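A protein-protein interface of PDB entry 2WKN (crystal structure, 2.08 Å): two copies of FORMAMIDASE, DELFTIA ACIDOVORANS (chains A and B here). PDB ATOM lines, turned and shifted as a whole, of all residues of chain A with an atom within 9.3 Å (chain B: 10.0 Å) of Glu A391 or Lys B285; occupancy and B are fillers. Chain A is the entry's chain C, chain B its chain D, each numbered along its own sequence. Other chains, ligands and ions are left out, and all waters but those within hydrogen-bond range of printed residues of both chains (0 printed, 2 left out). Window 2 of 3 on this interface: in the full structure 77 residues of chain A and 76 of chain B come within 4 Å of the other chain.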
ATOM      1  N   GLU A 337      -8.381   2.875  19.173  1.00  0.00           N
ATOM      2  CA  GLU A 337      -7.596   3.397  18.021  1.00  0.00           C
ATOM      3  C   GLU A 337      -8.460   4.095  17.011  1.00  0.00           C
ATOM      4  O   GLU A 337      -8.067   5.107  16.457  1.00  0.00           O
ATOM      5  CB  GLU A 337      -6.814   2.296  17.301  1.00  0.00           C
ATOM      6  CG  GLU A 337      -5.603   1.764  18.057  1.00  0.00           C
ATOM      7  CD  GLU A 337      -4.680   2.884  18.515  1.00  0.00           C
ATOM      8  OE1 GLU A 337      -4.229   3.675  17.648  1.00  0.00           O
ATOM      9  OE2 GLU A 337      -4.448   2.979  19.736  1.00  0.00           O
ATOM     10  N   TYR A 338      -9.648   3.547  16.776  1.00  0.00           N
ATOM     11  CA  TYR A 338     -10.604   4.148  15.839  1.00  0.00           C
ATOM     12  C   TYR A 338     -11.108   5.498  16.339  1.00  0.00           C
ATOM     13  O   TYR A 338     -11.140   6.494  15.590  1.00  0.00           O
ATOM     14  CB  TYR A 338     -11.768   3.179  15.601  1.00  0.00           C
ATOM     15  CG  TYR A 338     -12.717   3.601  14.503  1.00  0.00           C
ATOM     16  CD1 TYR A 338     -12.543   3.148  13.199  1.00  0.00           C
ATOM     17  CD2 TYR A 338     -13.783   4.455  14.766  1.00  0.00           C
ATOM     18  CE1 TYR A 338     -13.417   3.543  12.164  1.00  0.00           C
ATOM     19  CE2 TYR A 338     -14.671   4.852  13.742  1.00  0.00           C
ATOM     20  CZ  TYR A 338     -14.474   4.385  12.447  1.00  0.00           C
ATOM     21  OH  TYR A 338     -15.319   4.777  11.428  1.00  0.00           O
ATOM     22  N   LEU A 339     -11.519   5.543  17.595  1.00  0.00           N
ATOM     23  CA  LEU A 339     -12.022   6.790  18.173  1.00  0.00           C
ATOM     24  C   LEU A 339     -10.969   7.913  18.225  1.00  0.00           C
ATOM     25  O   LEU A 339     -11.291   9.059  17.966  1.00  0.00           O
ATOM     26  CB  LEU A 339     -12.612   6.536  19.554  1.00  0.00           C
ATOM     27  CG  LEU A 339     -14.022   5.895  19.564  1.00  0.00           C
ATOM     28  CD1 LEU A 339     -14.364   5.409  20.943  1.00  0.00           C
ATOM     29  CD2 LEU A 339     -15.091   6.866  19.082  1.00  0.00           C
ATOM     30  N   LYS A 340      -9.716   7.564  18.540  1.00  0.00           N
ATOM     31  CA  LYS A 340      -8.610   8.533  18.520  1.00  0.00           C
ATOM     32  C   LYS A 340      -8.449   9.282  17.201  1.00  0.00           C
ATOM     33  O   LYS A 340      -8.016  10.430  17.210  1.00  0.00           O
ATOM     34  CB  LYS A 340      -7.288   7.879  18.905  1.00  0.00           C
ATOM     35  CG  LYS A 340      -7.121   7.744  20.394  1.00  0.00           C
ATOM     36  CD  LYS A 340      -6.273   6.562  20.767  1.00  0.00           C
ATOM     37  CE  LYS A 340      -4.795   6.804  20.548  1.00  0.00           C
ATOM     38  NZ  LYS A 340      -4.030   5.666  21.145  1.00  0.00           N
ATOM     39  N   LYS A 341      -8.818   8.648  16.085  1.00  0.00           N
ATOM     40  CA  LYS A 341      -8.747   9.278  14.761  1.00  0.00           C
ATOM     41  C   LYS A 341      -9.749  10.402  14.596  1.00  0.00           C
ATOM     42  O   LYS A 341      -9.660  11.196  13.664  1.00  0.00           O
ATOM     43  CB  LYS A 341      -8.935   8.251  13.648  1.00  0.00           C
ATOM     44  CG  LYS A 341      -7.899   7.129  13.677  1.00  0.00           C
ATOM     45  CD  LYS A 341      -6.502   7.642  13.368  1.00  0.00           C
ATOM     46  CE  LYS A 341      -5.552   6.508  13.180  1.00  0.00           C
ATOM     47  NZ  LYS A 341      -4.160   6.993  13.025  1.00  0.00           N
ATOM     48  N   PHE A 342     -10.691  10.472  15.521  1.00  0.00           N
ATOM     49  CA  PHE A 342     -11.724  11.489  15.474  1.00  0.00           C
ATOM     50  C   PHE A 342     -11.411  12.607  16.451  1.00  0.00           C
ATOM     51  O   PHE A 342     -12.130  13.601  16.509  1.00  0.00           O
ATOM     52  CB  PHE A 342     -13.100  10.848  15.735  1.00  0.00           C
ATOM     53  CG  PHE A 342     -13.658  10.158  14.536  1.00  0.00           C
ATOM     54  CD1 PHE A 342     -13.408   8.815  14.316  1.00  0.00           C
ATOM     55  CD2 PHE A 342     -14.402  10.873  13.593  1.00  0.00           C
ATOM     56  CE1 PHE A 342     -13.912   8.164  13.179  1.00  0.00           C
ATOM     57  CE2 PHE A 342     -14.916  10.241  12.451  1.00  0.00           C
ATOM     58  CZ  PHE A 342     -14.676   8.882  12.244  1.00  0.00           C
ATOM     59  N   GLY A 343     -10.321  12.436  17.202  1.00  0.00           N
ATOM     60  CA  GLY A 343      -9.827  13.481  18.084  1.00  0.00           C
ATOM     61  C   GLY A 343      -9.981  13.227  19.561  1.00  0.00           C
ATOM     62  O   GLY A 343      -9.571  14.060  20.386  1.00  0.00           O
ATOM     63  N   ASN A 387     -19.030   7.049  11.097  1.00  0.00           N
ATOM     64  CA  ASN A 387     -18.953   5.921  10.184  1.00  0.00           C
ATOM     65  C   ASN A 387     -17.863   6.178   9.167  1.00  0.00           C
ATOM     66  O   ASN A 387     -17.589   7.348   8.847  1.00  0.00           O
ATOM     67  CB  ASN A 387     -20.316   5.666   9.492  1.00  0.00           C
ATOM     68  CG  ASN A 387     -21.326   4.986  10.423  1.00  0.00           C
ATOM     69  OD1 ASN A 387     -21.079   3.884  10.928  1.00  0.00           O
ATOM     70  ND2 ASN A 387     -22.444   5.650  10.678  1.00  0.00           N
ATOM     71  N   PRO A 388     -17.213   5.099   8.674  1.00  0.00           N
ATOM     72  CA  PRO A 388     -16.154   5.319   7.705  1.00  0.00           C
ATOM     73  C   PRO A 388     -16.716   5.800   6.372  1.00  0.00           C
ATOM     74  O   PRO A 388     -17.792   5.352   5.953  1.00  0.00           O
ATOM     75  CB  PRO A 388     -15.494   3.944   7.568  1.00  0.00           C
ATOM     76  CG  PRO A 388     -16.134   3.050   8.635  1.00  0.00           C
ATOM     77  CD  PRO A 388     -17.431   3.662   8.962  1.00  0.00           C
ATOM     78  N   THR A 389     -16.005   6.741   5.747  1.00  0.00           N
ATOM     79  CA  THR A 389     -16.344   7.267   4.421  1.00  0.00           C
ATOM     80  C   THR A 389     -15.128   7.172   3.498  1.00  0.00           C
ATOM     81  O   THR A 389     -14.047   6.820   3.949  1.00  0.00           O
ATOM     82  CB  THR A 389     -16.814   8.745   4.483  1.00  0.00           C
ATOM     83  OG1 THR A 389     -15.716   9.582   4.858  1.00  0.00           O
ATOM     84  CG2 THR A 389     -17.951   8.931   5.487  1.00  0.00           C
ATOM     85  N   ALA A 390     -15.313   7.488   2.216  1.00  0.00           N
ATOM     86  CA  ALA A 390     -14.230   7.462   1.234  1.00  0.00           C
ATOM     87  C   ALA A 390     -13.051   8.419   1.529  1.00  0.00           C
ATOM     88  O   ALA A 390     -11.903   8.015   1.402  1.00  0.00           O
ATOM     89  CB  ALA A 390     -14.773   7.688  -0.158  1.00  0.00           C
ATOM     90  N   GLU A 391     -13.304   9.668   1.909  1.00  0.00           N
ATOM     91  CA  GLU A 391     -12.177  10.607   2.109  1.00  0.00           C
ATOM     92  C   GLU A 391     -11.523  10.586   3.506  1.00  0.00           C
ATOM     93  O   GLU A 391     -10.503  11.262   3.733  1.00  0.00           O
ATOM     94  CB  GLU A 391     -12.521  12.043   1.680  1.00  0.00           C
ATOM     95  CG  GLU A 391     -13.648  12.698   2.441  1.00  0.00           C
ATOM     96  CD  GLU A 391     -14.985  12.478   1.777  1.00  0.00           C
ATOM     97  OE1 GLU A 391     -15.627  13.492   1.429  1.00  0.00           O
ATOM     98  OE2 GLU A 391     -15.390  11.302   1.591  1.00  0.00           O
ATOM     99  N   GLY A 392     -12.089   9.809   4.427  1.00  0.00           N
ATOM    100  CA  GLY A 392     -11.488   9.646   5.740  1.00  0.00           C
ATOM    101  C   GLY A 392     -12.119  10.518   6.811  1.00  0.00           C
ATOM    102  O   GLY A 392     -12.947  11.390   6.507  1.00  0.00           O
ATOM    103  N   PRO A 393     -11.723  10.299   8.073  1.00  0.00           N
ATOM    104  CA  PRO A 393     -12.299  10.997   9.229  1.00  0.00           C
ATOM    105  C   PRO A 393     -11.924  12.478   9.315  1.00  0.00           C
ATOM    106  O   PRO A 393     -10.759  12.822   9.110  1.00  0.00           O
ATOM    107  CB  PRO A 393     -11.691  10.248  10.420  1.00  0.00           C
ATOM    108  CG  PRO A 393     -10.432   9.674   9.912  1.00  0.00           C
ATOM    109  CD  PRO A 393     -10.630   9.385   8.464  1.00  0.00           C
ATOM    110  N   GLN A 394     -12.899  13.340   9.601  1.00  0.00           N
ATOM    111  CA  GLN A 394     -12.612  14.720  10.013  1.00  0.00           C
ATOM    112  C   GLN A 394     -12.438  14.764  11.529  1.00  0.00           C
ATOM    113  O   GLN A 394     -13.228  14.179  12.269  1.00  0.00           O
ATOM    114  CB  GLN A 394     -13.714  15.682   9.570  1.00  0.00           C
ATOM    115  CG  GLN A 394     -13.683  16.019   8.079  1.00  0.00           C
ATOM    116  CD  GLN A 394     -15.074  16.001   7.436  1.00  0.00           C
ATOM    117  OE1 GLN A 394     -16.084  15.769   8.111  1.00  0.00           O
ATOM    118  NE2 GLN A 394     -15.128  16.238   6.122  1.00  0.00           N
ATOM    119  N   LYS A 395     -11.392  15.451  11.977  1.00  0.00           N
ATOM    120  CA  LYS A 395     -11.021  15.509  13.385  1.00  0.00           C
ATOM    121  C   LYS A 395     -11.928  16.512  14.094  1.00  0.00           C
ATOM    122  O   LYS A 395     -11.522  17.644  14.361  1.00  0.00           O
ATOM    123  CB  LYS A 395      -9.543  15.910  13.508  1.00  0.00           C
ATOM    124  CG  LYS A 395      -8.841  15.504  14.807  1.00  0.00           C
ATOM    125  CD  LYS A 395      -8.327  14.054  14.788  1.00  0.00           C
ATOM    126  CE  LYS A 395      -7.051  13.867  13.974  1.00  0.00           C
ATOM    127  NZ  LYS A 395      -5.856  14.465  14.618  1.00  0.00           N
ATOM    128  N   GLY B  84      -3.131  -1.750   2.306  1.00  0.00           N
ATOM    129  CA  GLY B  84      -3.496  -0.610   3.148  1.00  0.00           C
ATOM    130  C   GLY B  84      -4.812   0.083   2.809  1.00  0.00           C
ATOM    131  O   GLY B  84      -5.220   1.013   3.503  1.00  0.00           O
ATOM    132  N   ASP B  85      -5.473  -0.363   1.741  1.00  0.00           N
ATOM    133  CA  ASP B  85      -6.842   0.063   1.468  1.00  0.00           C
ATOM    134  C   ASP B  85      -7.826  -0.669   2.405  1.00  0.00           C
ATOM    135  O   ASP B  85      -7.471  -1.667   3.061  1.00  0.00           O
ATOM    136  CB  ASP B  85      -7.230  -0.208   0.007  1.00  0.00           C
ATOM    137  CG  ASP B  85      -6.611   0.788  -0.978  1.00  0.00           C
ATOM    138  OD1 ASP B  85      -5.944   1.751  -0.548  1.00  0.00           O
ATOM    139  OD2 ASP B  85      -6.808   0.607  -2.202  1.00  0.00           O
ATOM    140  N   LEU B  86      -9.050  -0.161   2.479  1.00  0.00           N
ATOM    141  CA  LEU B  86     -10.153  -0.964   3.015  1.00  0.00           C
ATOM    142  C   LEU B  86     -11.032  -1.374   1.848  1.00  0.00           C
ATOM    143  O   LEU B  86     -11.372  -0.543   0.991  1.00  0.00           O
ATOM    144  CB  LEU B  86     -10.987  -0.200   4.061  1.00  0.00           C
ATOM    145  CG  LEU B  86     -10.345   0.131   5.411  1.00  0.00           C
ATOM    146  CD1 LEU B  86     -11.208   1.133   6.167  1.00  0.00           C
ATOM    147  CD2 LEU B  86     -10.123  -1.122   6.222  1.00  0.00           C
ATOM    148  N   VAL B  88     -14.626  -2.303   0.962  1.00  0.00           N
ATOM    149  CA  VAL B  88     -15.981  -2.188   1.478  1.00  0.00           C
ATOM    150  C   VAL B  88     -16.866  -3.197   0.776  1.00  0.00           C
ATOM    151  O   VAL B  88     -17.054  -3.103  -0.434  1.00  0.00           O
ATOM    152  CB  VAL B  88     -16.551  -0.770   1.263  1.00  0.00           C
ATOM    153  CG1 VAL B  88     -17.935  -0.627   1.953  1.00  0.00           C
ATOM    154  CG2 VAL B  88     -15.552   0.286   1.789  1.00  0.00           C
ATOM    155  N   LEU B 278     -14.017   0.751  -2.421  1.00  0.00           N
ATOM    156  CA  LEU B 278     -12.740   0.995  -1.757  1.00  0.00           C
ATOM    157  C   LEU B 278     -12.737   2.258  -0.924  1.00  0.00           C
ATOM    158  O   LEU B 278     -13.464   3.211  -1.229  1.00  0.00           O
ATOM    159  CB  LEU B 278     -11.611   1.093  -2.798  1.00  0.00           C
ATOM    160  CG  LEU B 278     -11.258  -0.116  -3.662  1.00  0.00           C
ATOM    161  CD1 LEU B 278     -10.273   0.325  -4.766  1.00  0.00           C
ATOM    162  CD2 LEU B 278     -10.681  -1.238  -2.824  1.00  0.00           C
ATOM    163  N   ILE B 279     -11.940   2.239   0.144  1.00  0.00           N
ATOM    164  CA  ILE B 279     -11.513   3.459   0.843  1.00  0.00           C
ATOM    165  C   ILE B 279      -9.996   3.525   0.729  1.00  0.00           C
ATOM    166  O   ILE B 279      -9.286   2.718   1.349  1.00  0.00           O
ATOM    167  CB  ILE B 279     -11.924   3.466   2.349  1.00  0.00           C
ATOM    168  CG1 ILE B 279     -13.447   3.375   2.496  1.00  0.00           C
ATOM    169  CG2 ILE B 279     -11.356   4.706   3.072  1.00  0.00           C
ATOM    170  CD1 ILE B 279     -13.953   3.427   3.936  1.00  0.00           C
ATOM    171  N   LYS B 280      -9.503   4.460  -0.089  1.00  0.00           N
ATOM    172  CA  LYS B 280      -8.059   4.549  -0.374  1.00  0.00           C
ATOM    173  C   LYS B 280      -7.283   4.898   0.893  1.00  0.00           C
ATOM    174  O   LYS B 280      -7.560   5.901   1.555  1.00  0.00           O
ATOM    175  CB  LYS B 280      -7.766   5.546  -1.506  1.00  0.00           C
ATOM    176  CG  LYS B 280      -8.389   5.208  -2.872  1.00  0.00           C
ATOM    177  CD  LYS B 280      -8.051   3.804  -3.348  1.00  0.00           C
ATOM    178  CE  LYS B 280      -6.596   3.645  -3.760  1.00  0.00           C
ATOM    179  NZ  LYS B 280      -6.320   2.300  -4.357  1.00  0.00           N
ATOM    180  N   GLY B 281      -6.331   4.042   1.242  1.00  0.00           N
ATOM    181  CA  GLY B 281      -5.574   4.176   2.481  1.00  0.00           C
ATOM    182  C   GLY B 281      -6.420   4.048   3.745  1.00  0.00           C
ATOM    183  O   GLY B 281      -6.098   4.630   4.799  1.00  0.00           O
ATOM    184  N   GLY B 282      -7.509   3.282   3.651  1.00  0.00           N
ATOM    185  CA  GLY B 282      -8.458   3.164   4.757  1.00  0.00           C
ATOM    186  C   GLY B 282      -7.825   2.699   6.051  1.00  0.00           C
ATOM    187  O   GLY B 282      -8.162   3.193   7.120  1.00  0.00           O
ATOM    188  N   MET B 283      -6.886   1.773   5.962  1.00  0.00           N
ATOM    189  CA  MET B 283      -6.295   1.180   7.174  1.00  0.00           C
ATOM    190  C   MET B 283      -5.615   2.168   8.130  1.00  0.00           C
ATOM    191  O   MET B 283      -5.795   2.092   9.351  1.00  0.00           O
ATOM    192  CB  MET B 283      -5.338   0.054   6.814  1.00  0.00           C
ATOM    193  CG  MET B 283      -6.034  -1.116   6.137  1.00  0.00           C
ATOM    194  SD  MET B 283      -4.948  -2.523   5.815  1.00  0.00           S
ATOM    195  CE  MET B 283      -4.166  -2.734   7.403  1.00  0.00           C
ATOM    196  N   ALA B 284      -4.837   3.092   7.575  1.00  0.00           N
ATOM    197  CA  ALA B 284      -4.131   4.083   8.400  1.00  0.00           C
ATOM    198  C   ALA B 284      -5.089   5.172   8.799  1.00  0.00           C
ATOM    199  O   ALA B 284      -5.047   5.657   9.930  1.00  0.00           O
ATOM    200  CB  ALA B 284      -2.944   4.672   7.635  1.00  0.00           C
ATOM    201  N   LYS B 285      -5.977   5.545   7.871  1.00  0.00           N
ATOM    202  CA  LYS B 285      -6.931   6.616   8.106  1.00  0.00           C
ATOM    203  C   LYS B 285      -7.794   6.354   9.346  1.00  0.00           C
ATOM    204  O   LYS B 285      -8.060   7.271  10.129  1.00  0.00           O
ATOM    205  CB  LYS B 285      -7.798   6.817   6.871  1.00  0.00           C
ATOM    206  CG  LYS B 285      -7.212   7.755   5.815  1.00  0.00           C
ATOM    207  CD  LYS B 285      -8.097   7.742   4.591  1.00  0.00           C
ATOM    208  CE  LYS B 285      -7.634   8.692   3.502  1.00  0.00           C
ATOM    209  NZ  LYS B 285      -8.528   8.513   2.310  1.00  0.00           N
ATOM    210  N   TYR B 286      -8.189   5.093   9.526  1.00  0.00           N
ATOM    211  CA  TYR B 286      -9.118   4.670  10.581  1.00  0.00           C
ATOM    212  C   TYR B 286      -8.477   3.735  11.631  1.00  0.00           C
ATOM    213  O   TYR B 286      -9.152   3.199  12.512  1.00  0.00           O
ATOM    214  CB  TYR B 286     -10.374   4.020   9.953  1.00  0.00           C
ATOM    215  CG  TYR B 286     -11.288   5.005   9.244  1.00  0.00           C
ATOM    216  CD1 TYR B 286     -11.337   5.058   7.865  1.00  0.00           C
ATOM    217  CD2 TYR B 286     -12.087   5.905   9.970  1.00  0.00           C
ATOM    218  CE1 TYR B 286     -12.174   5.960   7.212  1.00  0.00           C
ATOM    219  CE2 TYR B 286     -12.916   6.807   9.333  1.00  0.00           C
ATOM    220  CZ  TYR B 286     -12.957   6.830   7.952  1.00  0.00           C
ATOM    221  OH  TYR B 286     -13.765   7.743   7.317  1.00  0.00           O
ATOM    222  N   GLY B 287      -7.162   3.565  11.563  1.00  0.00           N
ATOM    223  CA  GLY B 287      -6.449   2.781  12.561  1.00  0.00           C
ATOM    224  C   GLY B 287      -6.969   1.356  12.617  1.00  0.00           C
ATOM    225  O   GLY B 287      -7.242   0.821  13.694  1.00  0.00           O
ATOM    226  N   ILE B 288      -7.098   0.748  11.442  1.00  0.00           N
ATOM    227  CA  ILE B 288      -7.688  -0.573  11.309  1.00  0.00           C
ATOM    228  C   ILE B 288      -6.648  -1.677  11.452  1.00  0.00           C
ATOM    229  O   ILE B 288      -5.653  -1.698  10.730  1.00  0.00           O
ATOM    230  CB  ILE B 288      -8.404  -0.730   9.947  1.00  0.00           C
ATOM    231  CG1 ILE B 288      -9.504   0.323   9.773  1.00  0.00           C
ATOM    232  CG2 ILE B 288      -8.953  -2.163   9.769  1.00  0.00           C
ATOM    233  CD1 ILE B 288     -10.612   0.288  10.796  1.00  0.00           C
ATOM    234  N   LYS B 289      -6.887  -2.588  12.389  1.00  0.00           N
ATOM    235  CA  LYS B 289      -6.136  -3.830  12.469  1.00  0.00           C
ATOM    236  C   LYS B 289      -7.034  -4.995  12.005  1.00  0.00           C
ATOM    237  O   LYS B 289      -6.832  -5.530  10.920  1.00  0.00           O
ATOM    238  CB  LYS B 289      -5.594  -4.041  13.879  1.00  0.00           C
ATOM    239  CG  LYS B 289      -4.708  -5.258  14.044  1.00  0.00           C
ATOM    240  CD  LYS B 289      -4.041  -5.252  15.399  1.00  0.00           C
ATOM    241  CE  LYS B 289      -3.544  -6.638  15.761  1.00  0.00           C
ATOM    242  NZ  LYS B 289      -3.154  -6.735  17.201  1.00  0.00           N
ATOM    243  N   ILE B 292     -13.882  -4.223  10.570  1.00  0.00           N
ATOM    244  CA  ILE B 292     -14.995  -3.645  11.289  1.00  0.00           C
ATOM    245  C   ILE B 292     -16.195  -3.736  10.377  1.00  0.00           C
ATOM    246  O   ILE B 292     -16.039  -3.844   9.162  1.00  0.00           O
ATOM    247  CB  ILE B 292     -14.750  -2.170  11.713  1.00  0.00           C
ATOM    248  CG1 ILE B 292     -14.659  -1.250  10.502  1.00  0.00           C
ATOM    249  CG2 ILE B 292     -13.500  -2.071  12.586  1.00  0.00           C
ATOM    250  CD1 ILE B 292     -14.337   0.191  10.875  1.00  0.00           C
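The side-chain amino group (NZ) of Lys A341 lies close to the backbone carbonyl oxygen (O) of Ala B284, 3.5 Å away.
The backbone nitrogen (N) of Pro A393 sits close to the side-chain hydroxyl (OH) of Tyr B286.
The backbone NH (N) of Thr A389 is in hydrogen-bond range of the side-chain hydroxyl (OH) of Tyr B286 (2.9 Å).
The backbone carbonyl oxygen (O) of Leu B86 sits at hydrogen-bond distance from the backbone NH (N) of Ile B279 (3.0 Å).
The side-chain amino group of Lys B285 lies within hydrogen-bond range of the backbone carbonyl oxygen of Lys B280 (2.9 Å).
The side-chain amino group of Lys A340 lies within salt-bridge range of the side-chain carboxylate of Glu A337, at 3.1 Å.
Among the printed residues, pairs that only touch across the chains: Glu A337 with Gly B287 (3.9 Å), Tyr A338 with Tyr B286 (3.5 Å), Tyr A338 with Ile B292 (3.7 Å), Lys A341 with Lys B285 (3.6 Å), Lys A341 with Gly B287 (3.7 Å), Phe A342 with Tyr B286 (3.98 Å), Pro A388 with Ile B279 (3.98 Å), Pro A388 with Tyr B286 (3.4 Å), Thr A389 with Ile B279 (3.4 Å), Ala A390 with Ile B279 (3.7 Å), Ala A390 with Lys B285 (3.5 Å), Glu A391 with Lys B285 (3.7 Å), Gly A392 with Tyr B286 (3.3 Å) and Pro A393 with Lys B285 (3.4 Å).
Glu A391 touches just one residue of chain B: Lys B285 (3.7 Å).
Lys B285 touches just these residues of chain A: Lys A341, Ala A390, Glu A391 and Pro A393.
Ala A390 touches just these residues of chain B: Ile B279 and Lys B285.
Gly A392 touches just one residue of chain B: Tyr B286 (3.3 Å).
No residue of chain A comes within 4 Å of Gly B281.
Printed residues of chain A within 4 Å of Ala B284: Lys A341 (3.4 Å).
Of the printed residues of chain A, Tyr B286 touches Tyr A338 (3.5 Å), Phe A342 (3.98 Å), Pro A388 (3.4 Å), Thr A389 (2.9 Å), Gly A392 (3.3 Å) and Pro A393 (3.4 Å).
Of the printed residues of chain B, Phe A342 touches Tyr B286 (3.98 Å).
Printed residues of chain B within 4 Å of Tyr A338: Tyr B286 and Ile B292.
Printed residues of chain A within 4 Å of Gly B287: Glu A337 (3.9 Å) and Lys A341 (3.7 Å).
Of the printed residues of chain B, Pro A388 touches Ile B279 (3.98 Å) and Tyr B286 (3.4 Å).
Leu A339 touches none of the printed residues of chain B.
Gly A343 touches none of the printed residues of chain B.
The nearest residue of chain A that does not touch Lys B285 is Gly A392 (4.1 Å).
Of the 16 printed residues of chain A, 10 touch a printed residue of chain B.
Among the printed residues, 17 pairs touch across the chains.
Among the printed residues, no Asp or Glu carboxylate lies within 4 Å of a Lys or Arg side-chain nitrogen of the other chain.
No position is printed for both chains.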
